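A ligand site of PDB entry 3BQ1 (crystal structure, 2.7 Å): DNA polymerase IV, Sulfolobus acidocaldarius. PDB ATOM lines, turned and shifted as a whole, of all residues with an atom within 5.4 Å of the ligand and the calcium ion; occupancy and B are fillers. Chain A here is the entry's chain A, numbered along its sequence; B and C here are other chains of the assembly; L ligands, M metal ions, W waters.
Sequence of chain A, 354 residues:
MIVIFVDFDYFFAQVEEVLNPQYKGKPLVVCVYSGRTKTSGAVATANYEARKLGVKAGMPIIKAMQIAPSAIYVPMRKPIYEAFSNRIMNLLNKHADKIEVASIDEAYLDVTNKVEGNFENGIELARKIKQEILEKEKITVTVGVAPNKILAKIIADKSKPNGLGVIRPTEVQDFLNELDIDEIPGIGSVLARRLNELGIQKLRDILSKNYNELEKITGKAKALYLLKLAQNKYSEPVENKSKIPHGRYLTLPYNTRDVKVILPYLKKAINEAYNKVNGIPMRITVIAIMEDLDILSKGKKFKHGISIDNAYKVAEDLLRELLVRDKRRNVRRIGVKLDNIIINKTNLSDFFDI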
ATOM      1  N   ASP A   7      14.890 -13.386 -17.207  1.00  0.00           N
ATOM      2  CA  ASP A   7      15.908 -13.366 -18.229  1.00  0.00           C
ATOM      3  C   ASP A   7      17.262 -13.427 -17.535  1.00  0.00           C
ATOM      4  O   ASP A   7      17.561 -12.605 -16.663  1.00  0.00           O
ATOM      5  CB  ASP A   7      15.775 -12.103 -19.072  1.00  0.00           C
ATOM      6  CG  ASP A   7      16.839 -12.015 -20.154  1.00  0.00           C
ATOM      7  OD1 ASP A   7      16.504 -11.628 -21.303  1.00  0.00           O
ATOM      8  OD2 ASP A   7      18.023 -12.345 -19.853  1.00  0.00           O
ATOM      9  N   PHE A   8      18.077 -14.405 -17.921  1.00  0.00           N
ATOM     10  CA  PHE A   8      19.350 -14.634 -17.226  1.00  0.00           C
ATOM     11  C   PHE A   8      20.369 -13.599 -17.682  1.00  0.00           C
ATOM     12  O   PHE A   8      20.516 -13.373 -18.892  1.00  0.00           O
ATOM     13  CB  PHE A   8      19.902 -16.063 -17.435  1.00  0.00           C
ATOM     14  CG  PHE A   8      18.887 -17.167 -17.231  1.00  0.00           C
ATOM     15  CD1 PHE A   8      19.067 -18.402 -17.849  1.00  0.00           C
ATOM     16  CD2 PHE A   8      17.759 -16.990 -16.417  1.00  0.00           C
ATOM     17  CE1 PHE A   8      18.145 -19.451 -17.678  1.00  0.00           C
ATOM     18  CE2 PHE A   8      16.826 -18.019 -16.247  1.00  0.00           C
ATOM     19  CZ  PHE A   8      17.019 -19.252 -16.870  1.00  0.00           C
ATOM     20  N   ASP A   9      21.052 -12.990 -16.715  1.00  0.00           N
ATOM     21  CA  ASP A   9      22.003 -11.894 -16.956  1.00  0.00           C
ATOM     22  C   ASP A   9      23.268 -12.393 -17.652  1.00  0.00           C
ATOM     23  O   ASP A   9      23.912 -13.325 -17.161  1.00  0.00           O
ATOM     24  CB  ASP A   9      22.404 -11.218 -15.640  1.00  0.00           C
ATOM     25  CG  ASP A   9      21.260 -10.439 -15.004  1.00  0.00           C
ATOM     26  OD1 ASP A   9      21.200 -10.378 -13.752  1.00  0.00           O
ATOM     27  OD2 ASP A   9      20.411  -9.889 -15.754  1.00  0.00           O
ATOM     28  N   TYR A  10      23.624 -11.775 -18.776  1.00  0.00           N
ATOM     29  CA  TYR A  10      24.798 -12.179 -19.560  1.00  0.00           C
ATOM     30  C   TYR A  10      25.130 -13.703 -19.414  1.00  0.00           C
ATOM     31  O   TYR A  10      26.224 -14.101 -18.978  1.00  0.00           O
ATOM     32  CB  TYR A  10      25.991 -11.249 -19.288  1.00  0.00           C
ATOM     33  CG  TYR A  10      26.521 -11.308 -17.875  1.00  0.00           C
ATOM     34  CD1 TYR A  10      27.637 -12.090 -17.569  1.00  0.00           C
ATOM     35  CD2 TYR A  10      25.913 -10.588 -16.847  1.00  0.00           C
ATOM     36  CE1 TYR A  10      28.138 -12.167 -16.272  1.00  0.00           C
ATOM     37  CE2 TYR A  10      26.399 -10.654 -15.546  1.00  0.00           C
ATOM     38  CZ  TYR A  10      27.511 -11.449 -15.269  1.00  0.00           C
ATOM     39  OH  TYR A  10      28.022 -11.526 -13.987  1.00  0.00           O
ATOM     40  N   PHE A  11      24.168 -14.534 -19.799  1.00  0.00           N
ATOM     41  CA  PHE A  11      24.150 -15.924 -19.372  1.00  0.00           C
ATOM     42  C   PHE A  11      25.451 -16.713 -19.580  1.00  0.00           C
ATOM     43  O   PHE A  11      26.023 -17.217 -18.613  1.00  0.00           O
ATOM     44  CB  PHE A  11      22.944 -16.654 -19.983  1.00  0.00           C
ATOM     45  CG  PHE A  11      22.720 -18.024 -19.429  1.00  0.00           C
ATOM     46  CD1 PHE A  11      22.746 -18.255 -18.057  1.00  0.00           C
ATOM     47  CD2 PHE A  11      22.464 -19.092 -20.287  1.00  0.00           C
ATOM     48  CE1 PHE A  11      22.533 -19.526 -17.545  1.00  0.00           C
ATOM     49  CE2 PHE A  11      22.260 -20.358 -19.803  1.00  0.00           C
ATOM     50  CZ  PHE A  11      22.298 -20.591 -18.424  1.00  0.00           C
ATOM     51  N   PHE A  12      25.922 -16.809 -20.830  1.00  0.00           N
ATOM     52  CA  PHE A  12      27.074 -17.652 -21.139  1.00  0.00           C
ATOM     53  C   PHE A  12      28.301 -17.220 -20.345  1.00  0.00           C
ATOM     54  O   PHE A  12      28.976 -18.037 -19.696  1.00  0.00           O
ATOM     55  CB  PHE A  12      27.403 -17.691 -22.635  1.00  0.00           C
ATOM     56  CG  PHE A  12      26.297 -18.245 -23.504  1.00  0.00           C
ATOM     57  CD1 PHE A  12      25.195 -18.901 -22.947  1.00  0.00           C
ATOM     58  CD2 PHE A  12      26.372 -18.137 -24.875  1.00  0.00           C
ATOM     59  CE1 PHE A  12      24.179 -19.410 -23.777  1.00  0.00           C
ATOM     60  CE2 PHE A  12      25.369 -18.645 -25.711  1.00  0.00           C
ATOM     61  CZ  PHE A  12      24.276 -19.284 -25.162  1.00  0.00           C
ATOM     62  N   VAL A  32      32.258 -17.362 -30.258  1.00  0.00           N
ATOM     63  CA  VAL A  32      31.654 -18.350 -31.134  1.00  0.00           C
ATOM     64  C   VAL A  32      32.383 -18.304 -32.454  1.00  0.00           C
ATOM     65  O   VAL A  32      32.599 -17.225 -33.016  1.00  0.00           O
ATOM     66  CB  VAL A  32      30.114 -18.106 -31.316  1.00  0.00           C
ATOM     67  CG1 VAL A  32      29.785 -16.640 -31.594  1.00  0.00           C
ATOM     68  CG2 VAL A  32      29.543 -19.011 -32.408  1.00  0.00           C
ATOM     69  N   VAL A  43      31.956 -12.343 -30.988  1.00  0.00           N
ATOM     70  CA  VAL A  43      31.554 -12.307 -29.583  1.00  0.00           C
ATOM     71  C   VAL A  43      30.156 -12.916 -29.417  1.00  0.00           C
ATOM     72  O   VAL A  43      29.179 -12.451 -30.033  1.00  0.00           O
ATOM     73  CB  VAL A  43      31.564 -10.871 -29.023  1.00  0.00           C
ATOM     74  CG1 VAL A  43      30.966 -10.832 -27.613  1.00  0.00           C
ATOM     75  CG2 VAL A  43      32.967 -10.339 -28.991  1.00  0.00           C
ATOM     76  N   ALA A  44      30.066 -13.943 -28.587  1.00  0.00           N
ATOM     77  CA  ALA A  44      28.775 -14.516 -28.230  1.00  0.00           C
ATOM     78  C   ALA A  44      28.208 -13.805 -27.004  1.00  0.00           C
ATOM     79  O   ALA A  44      27.075 -13.320 -27.021  1.00  0.00           O
ATOM     80  CB  ALA A  44      28.885 -15.994 -28.002  1.00  0.00           C
ATOM     81  N   THR A  45      29.000 -13.712 -25.933  1.00  0.00           N
ATOM     82  CA  THR A  45      28.601 -13.005 -24.721  1.00  0.00           C
ATOM     83  C   THR A  45      29.801 -12.362 -24.040  1.00  0.00           C
ATOM     84  O   THR A  45      30.857 -12.989 -23.918  1.00  0.00           O
ATOM     85  CB  THR A  45      27.947 -13.965 -23.736  1.00  0.00           C
ATOM     86  OG1 THR A  45      26.886 -14.671 -24.382  1.00  0.00           O
ATOM     87  CG2 THR A  45      27.406 -13.202 -22.501  1.00  0.00           C
ATOM     88  N   TYR A  48      29.944  -7.912 -17.774  1.00  0.00           N
ATOM     89  CA  TYR A  48      29.734  -6.478 -17.712  1.00  0.00           C
ATOM     90  C   TYR A  48      30.995  -5.636 -17.681  1.00  0.00           C
ATOM     91  O   TYR A  48      30.978  -4.474 -18.099  1.00  0.00           O
ATOM     92  CB  TYR A  48      28.730  -6.093 -16.626  1.00  0.00           C
ATOM     93  CG  TYR A  48      27.305  -6.098 -17.160  1.00  0.00           C
ATOM     94  CD1 TYR A  48      26.646  -4.897 -17.516  1.00  0.00           C
ATOM     95  CD2 TYR A  48      26.621  -7.312 -17.336  1.00  0.00           C
ATOM     96  CE1 TYR A  48      25.326  -4.907 -18.014  1.00  0.00           C
ATOM     97  CE2 TYR A  48      25.304  -7.335 -17.833  1.00  0.00           C
ATOM     98  CZ  TYR A  48      24.672  -6.139 -18.166  1.00  0.00           C
ATOM     99  OH  TYR A  48      23.369  -6.200 -18.647  1.00  0.00           O
ATOM    100  N   ARG A  51      31.530  -5.469 -21.336  1.00  0.00           N
ATOM    101  CA  ARG A  51      30.508  -4.598 -21.930  1.00  0.00           C
ATOM    102  C   ARG A  51      30.789  -3.129 -21.639  1.00  0.00           C
ATOM    103  O   ARG A  51      30.421  -2.256 -22.423  1.00  0.00           O
ATOM    104  CB  ARG A  51      29.106  -4.965 -21.447  1.00  0.00           C
ATOM    105  CG  ARG A  51      28.632  -6.282 -21.954  1.00  0.00           C
ATOM    106  CD  ARG A  51      27.254  -6.639 -21.449  1.00  0.00           C
ATOM    107  NE  ARG A  51      26.915  -7.995 -21.903  1.00  0.00           N
ATOM    108  CZ  ARG A  51      25.691  -8.503 -21.984  1.00  0.00           C
ATOM    109  NH1 ARG A  51      24.627  -7.780 -21.635  1.00  0.00           N
ATOM    110  NH2 ARG A  51      25.540  -9.741 -22.415  1.00  0.00           N
ATOM    111  N   ALA A  57      27.878  -8.185 -28.220  1.00  0.00           N
ATOM    112  CA  ALA A  57      27.663  -9.459 -28.916  1.00  0.00           C
ATOM    113  C   ALA A  57      27.663  -9.236 -30.421  1.00  0.00           C
ATOM    114  O   ALA A  57      27.206  -8.203 -30.897  1.00  0.00           O
ATOM    115  CB  ALA A  57      26.374 -10.098 -28.464  1.00  0.00           C
ATOM    116  N   GLY A  58      28.182 -10.214 -31.163  1.00  0.00           N
ATOM    117  CA  GLY A  58      28.218 -10.167 -32.625  1.00  0.00           C
ATOM    118  C   GLY A  58      29.417  -9.417 -33.158  1.00  0.00           C
ATOM    119  O   GLY A  58      29.751  -9.511 -34.362  1.00  0.00           O
ATOM    120  N   ASP A 105      17.684 -18.733 -22.076  1.00  0.00           N
ATOM    121  CA  ASP A 105      17.809 -17.865 -20.918  1.00  0.00           C
ATOM    122  C   ASP A 105      16.583 -17.009 -20.593  1.00  0.00           C
ATOM    123  O   ASP A 105      16.626 -16.147 -19.712  1.00  0.00           O
ATOM    124  CB  ASP A 105      19.068 -17.000 -21.016  1.00  0.00           C
ATOM    125  CG  ASP A 105      18.929 -15.852 -22.016  1.00  0.00           C
ATOM    126  OD1 ASP A 105      18.317 -16.041 -23.093  1.00  0.00           O
ATOM    127  OD2 ASP A 105      19.448 -14.756 -21.715  1.00  0.00           O
ATOM    128  N   GLU A 106      15.465 -17.270 -21.278  1.00  0.00           N
ATOM    129  CA  GLU A 106      14.251 -16.482 -21.118  1.00  0.00           C
ATOM    130  C   GLU A 106      13.032 -17.369 -20.897  1.00  0.00           C
ATOM    131  O   GLU A 106      12.790 -18.296 -21.687  1.00  0.00           O
ATOM    132  CB  GLU A 106      14.014 -15.579 -22.335  1.00  0.00           C
ATOM    133  CG  GLU A 106      15.174 -14.609 -22.632  1.00  0.00           C
ATOM    134  CD  GLU A 106      14.895 -13.673 -23.807  1.00  0.00           C
ATOM    135  OE1 GLU A 106      13.981 -13.960 -24.605  1.00  0.00           O
ATOM    136  OE2 GLU A 106      15.621 -12.652 -23.932  1.00  0.00           O
ATOM    137  N   LYS A 160      17.831  -4.389 -16.595  1.00  0.00           N
ATOM    138  CA  LYS A 160      19.035  -5.216 -16.571  1.00  0.00           C
ATOM    139  C   LYS A 160      20.279  -4.430 -16.126  1.00  0.00           C
ATOM    140  O   LYS A 160      20.372  -3.237 -16.386  1.00  0.00           O
ATOM    141  CB  LYS A 160      19.291  -5.803 -17.956  1.00  0.00           C
ATOM    142  CG  LYS A 160      18.444  -6.986 -18.329  1.00  0.00           C
ATOM    143  CD  LYS A 160      18.751  -7.381 -19.753  1.00  0.00           C
ATOM    144  CE  LYS A 160      17.849  -8.494 -20.200  1.00  0.00           C
ATOM    145  NZ  LYS A 160      18.244  -9.023 -21.537  1.00  0.00           N
ATOM    146  P    DC B   3      28.674  -6.053 -40.254  1.00  0.00           P
ATOM    147  OP1  DC B   3      29.153  -6.841 -41.411  1.00  0.00           O
ATOM    148  OP2  DC B   3      27.198  -5.896 -40.116  1.00  0.00           O
ATOM    149  O5'  DC B   3      29.297  -6.681 -38.906  1.00  0.00           O
ATOM    150  C5'  DC B   3      30.520  -7.435 -38.866  1.00  0.00           C
ATOM    151  C4'  DC B   3      30.288  -8.908 -38.571  1.00  0.00           C
ATOM    152  O4'  DC B   3      29.464  -9.096 -37.386  1.00  0.00           O
ATOM    153  C3'  DC B   3      29.570  -9.697 -39.677  1.00  0.00           C
ATOM    154  O3'  DC B   3      30.166 -10.979 -39.821  1.00  0.00           O
ATOM    155  C2'  DC B   3      28.119  -9.781 -39.193  1.00  0.00           C
ATOM    156  C1'  DC B   3      28.312  -9.888 -37.689  1.00  0.00           C
ATOM    157  N1   DC B   3      27.164  -9.441 -36.817  1.00  0.00           N
ATOM    158  C2   DC B   3      26.689 -10.283 -35.794  1.00  0.00           C
ATOM    159  O2   DC B   3      27.213 -11.395 -35.639  1.00  0.00           O
ATOM    160  N3   DC B   3      25.671  -9.853 -35.005  1.00  0.00           N
ATOM    161  C4   DC B   3      25.127  -8.649 -35.199  1.00  0.00           C
ATOM    162  N4   DC B   3      24.130  -8.285 -34.391  1.00  0.00           N
ATOM    163  C5   DC B   3      25.591  -7.772 -36.215  1.00  0.00           C
ATOM    164  C6   DC B   3      26.601  -8.202 -36.989  1.00  0.00           C
ATOM    165  P    DC B   4      29.972 -11.829 -41.167  1.00  0.00           P
ATOM    166  OP1  DC B   4      31.356 -12.155 -41.613  1.00  0.00           O
ATOM    167  OP2  DC B   4      29.046 -11.124 -42.071  1.00  0.00           O
ATOM    168  O5'  DC B   4      29.222 -13.161 -40.690  1.00  0.00           O
ATOM    169  C5'  DC B   4      29.964 -14.252 -40.152  1.00  0.00           C
ATOM    170  C4'  DC B   4      29.039 -15.248 -39.468  1.00  0.00           C
ATOM    171  O4'  DC B   4      28.134 -14.551 -38.575  1.00  0.00           O
ATOM    172  C3'  DC B   4      28.166 -16.064 -40.410  1.00  0.00           C
ATOM    173  O3'  DC B   4      28.319 -17.452 -40.056  1.00  0.00           O
ATOM    174  C2'  DC B   4      26.751 -15.536 -40.173  1.00  0.00           C
ATOM    175  C1'  DC B   4      26.827 -15.063 -38.731  1.00  0.00           C
ATOM    176  N1   DC B   4      25.855 -13.996 -38.325  1.00  0.00           N
ATOM    177  C2   DC B   4      25.018 -14.199 -37.208  1.00  0.00           C
ATOM    178  O2   DC B   4      25.086 -15.259 -36.559  1.00  0.00           O
ATOM    179  N3   DC B   4      24.143 -13.210 -36.843  1.00  0.00           N
ATOM    180  C4   DC B   4      24.090 -12.076 -37.552  1.00  0.00           C
ATOM    181  N4   DC B   4      23.224 -11.139 -37.155  1.00  0.00           N
ATOM    182  C5   DC B   4      24.933 -11.838 -38.692  1.00  0.00           C
ATOM    183  C6   DC B   4      25.787 -12.813 -39.029  1.00  0.00           C
ATOM    184  P    DG C  10      15.355 -13.393 -29.487  1.00  0.00           P
ATOM    185  OP1  DG C  10      14.134 -14.180 -29.147  1.00  0.00           O
ATOM    186  OP2  DG C  10      15.756 -12.143 -28.774  1.00  0.00           O
ATOM    187  O5'  DG C  10      16.641 -14.327 -29.381  1.00  0.00           O
ATOM    188  C5'  DG C  10      16.550 -15.729 -29.647  1.00  0.00           C
ATOM    189  C4'  DG C  10      17.945 -16.297 -29.641  1.00  0.00           C
ATOM    190  O4'  DG C  10      18.660 -15.662 -30.721  1.00  0.00           O
ATOM    191  C3'  DG C  10      18.692 -15.988 -28.351  1.00  0.00           C
ATOM    192  O3'  DG C  10      19.338 -17.163 -27.863  1.00  0.00           O
ATOM    193  C2'  DG C  10      19.686 -14.900 -28.755  1.00  0.00           C
ATOM    194  C1'  DG C  10      19.872 -15.123 -30.252  1.00  0.00           C
ATOM    195  N9   DG C  10      20.189 -13.914 -31.038  1.00  0.00           N
ATOM    196  C8   DG C  10      19.729 -12.638 -30.827  1.00  0.00           C
ATOM    197  N7   DG C  10      20.190 -11.766 -31.684  1.00  0.00           N
ATOM    198  C5   DG C  10      21.006 -12.516 -32.535  1.00  0.00           C
ATOM    199  C6   DG C  10      21.778 -12.118 -33.666  1.00  0.00           C
ATOM    200  O6   DG C  10      21.903 -10.993 -34.168  1.00  0.00           O
ATOM    201  N1   DG C  10      22.465 -13.200 -34.227  1.00  0.00           N
ATOM    202  C2   DG C  10      22.412 -14.496 -33.755  1.00  0.00           C
ATOM    203  N2   DG C  10      23.143 -15.429 -34.419  1.00  0.00           N
ATOM    204  N3   DG C  10      21.693 -14.879 -32.707  1.00  0.00           N
ATOM    205  C4   DG C  10      21.016 -13.837 -32.139  1.00  0.00           C
HETATM  206  P1  LIG L   1      21.245 -10.113 -22.354  1.00  0.00           P
HETATM  207  O1  LIG L   1      20.208 -10.467 -23.418  1.00  0.00           O
HETATM  208  O2  LIG L   1      20.974 -10.525 -20.907  1.00  0.00           O
HETATM  209  O3  LIG L   1      21.700  -8.675 -22.443  1.00  0.00           O
HETATM  210  O4  LIG L   1      22.573 -10.956 -22.760  1.00  0.00           O
HETATM  211  P2  LIG L   1      22.595 -12.560 -22.897  1.00  0.00           P
HETATM  212  O5  LIG L   1      23.905 -12.969 -23.513  1.00  0.00           O
HETATM  213  O6  LIG L   1      22.280 -13.114 -21.528  1.00  0.00           O
HETATM  214  O7  LIG L   1      21.376 -12.990 -23.874  1.00  0.00           O
HETATM  215  P3  LIG L   1      21.161 -12.824 -25.485  1.00  0.00           P
HETATM  216  O8  LIG L   1      21.204 -11.329 -25.805  1.00  0.00           O
HETATM  217  O9  LIG L   1      19.890 -13.614 -25.772  1.00  0.00           O
HETATM  218  O10 LIG L   1      22.320 -13.634 -26.287  1.00  0.00           O
HETATM  219  C1  LIG L   1      22.423 -15.045 -26.130  1.00  0.00           C
HETATM  220  C2  LIG L   1      23.199 -15.806 -27.219  1.00  0.00           C
HETATM  221  O11 LIG L   1      22.742 -15.577 -28.564  1.00  0.00           O
HETATM  222  C3  LIG L   1      24.688 -15.494 -27.221  1.00  0.00           C
HETATM  223  C4  LIG L   1      25.086 -15.481 -28.682  1.00  0.00           C
HETATM  224  C5  LIG L   1      23.812 -15.248 -29.445  1.00  0.00           C
HETATM  225  N1  LIG L   1      23.649 -13.819 -29.805  1.00  0.00           N
HETATM  226  C6  LIG L   1      22.952 -12.871 -29.148  1.00  0.00           C
HETATM  227  N2  LIG L   1      23.014 -11.661 -29.802  1.00  0.00           N
HETATM  228  C7  LIG L   1      23.773 -11.844 -30.894  1.00  0.00           C
HETATM  229  C8  LIG L   1      24.260 -11.007 -32.010  1.00  0.00           C
HETATM  230  O12 LIG L   1      23.962  -9.790 -32.099  1.00  0.00           O
HETATM  231  N3  LIG L   1      25.023 -11.611 -32.934  1.00  0.00           N
HETATM  232  C9  LIG L   1      25.363 -12.918 -32.873  1.00  0.00           C
HETATM  233  N4  LIG L   1      26.143 -13.451 -33.835  1.00  0.00           N
HETATM  234  N5  LIG L   1      24.972 -13.736 -31.881  1.00  0.00           N
HETATM  235  C10 LIG L   1      24.185 -13.260 -30.890  1.00  0.00           C
HETATM  236 CA    CA M   1      19.989 -12.626 -21.030  1.00  0.00          CA
HETATM  237  O   HOH W   1      19.467 -10.218 -18.186  1.00  0.00           O
HETATM  238  O   HOH W   2      22.633 -10.032 -27.570  1.00  0.00           O
HETATM  239  O   HOH W   3      18.249 -12.800 -23.444  1.00  0.00           O
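N3 of DC 3 of chain B lies within hydrogen-bond range of N3 of the ligand, at 2.8 Å.
An oxygen (O6) of the ligand sits close to the backbone NH (N) of Phe 11, at 2.9 Å.
The side-chain amino group (NZ) of Lys 160 is in salt-bridge range of an oxygen (O1) of the ligand, at 3.1 Å.
N1 of DG 10 of chain C lies close to N3 of the ligand (3.3 Å).
NH1 of Arg 51 lies within salt-bridge range of O3 of the ligand.
N of Tyr 10 of chain A lies close to O6 of the ligand, 3.3 Å away.
O2 of DC 4 of chain B sits at hydrogen-bond distance from N4 of the ligand (3.4 Å).
OD1 of Asp 7 is in salt-bridge range of NZ of Lys 160 (3.1 Å).
N of Gly 58 sits at hydrogen-bond distance from O of Val 43, 2.7 Å away.
Residues that only touch the ligand: Phe 12 (3.6 Å), Ala 44 (3.2 Å), Thr 45 (3.5 Å), Ala 57 (3.8 Å) and Gly 58 (3.5 Å).
Hydrophobic or aromatic side chains within 4 Å of the ligand: Phe 11, Phe 12, Ala 44 and Ala 57.
15 residues have an atom within 4 Å of the ligand: Asp 7, Phe 8, Tyr 10 of chain A, Phe 11, Phe 12, Ala 44, Thr 45, Arg 51, Ala 57, Gly 58, Asp 105, Lys 160, DC 3 of chain B, DC 4 of chain B and DG 10 of chain C.
Three residues have an atom within 4 Å of the calcium ion: Asp 7, Phe 8 and Asp 105.
OD2 of Asp 105 is bound to the calcium ion (2.3 Å).
OD2 of Asp 7 binds the calcium ion (2.3 Å).
O2 of the ligand is bound to the calcium ion (2.3 Å).
The calcium ion is bound by the backbone carbonyl oxygen (O) of Phe 8, at 2.3 Å.
The calcium ion is bound by an oxygen (O6) of the ligand, 2.4 Å away.
The calcium ion has five donor atoms within binding distance.
Slightly farther from the calcium ion lies water W3 (3.0 Å).
Water W1 bridges the side-chain carboxylate of Asp 9 (2.6 Å) and the backbone carbonyl oxygen of Asp 7 (3.4 Å).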
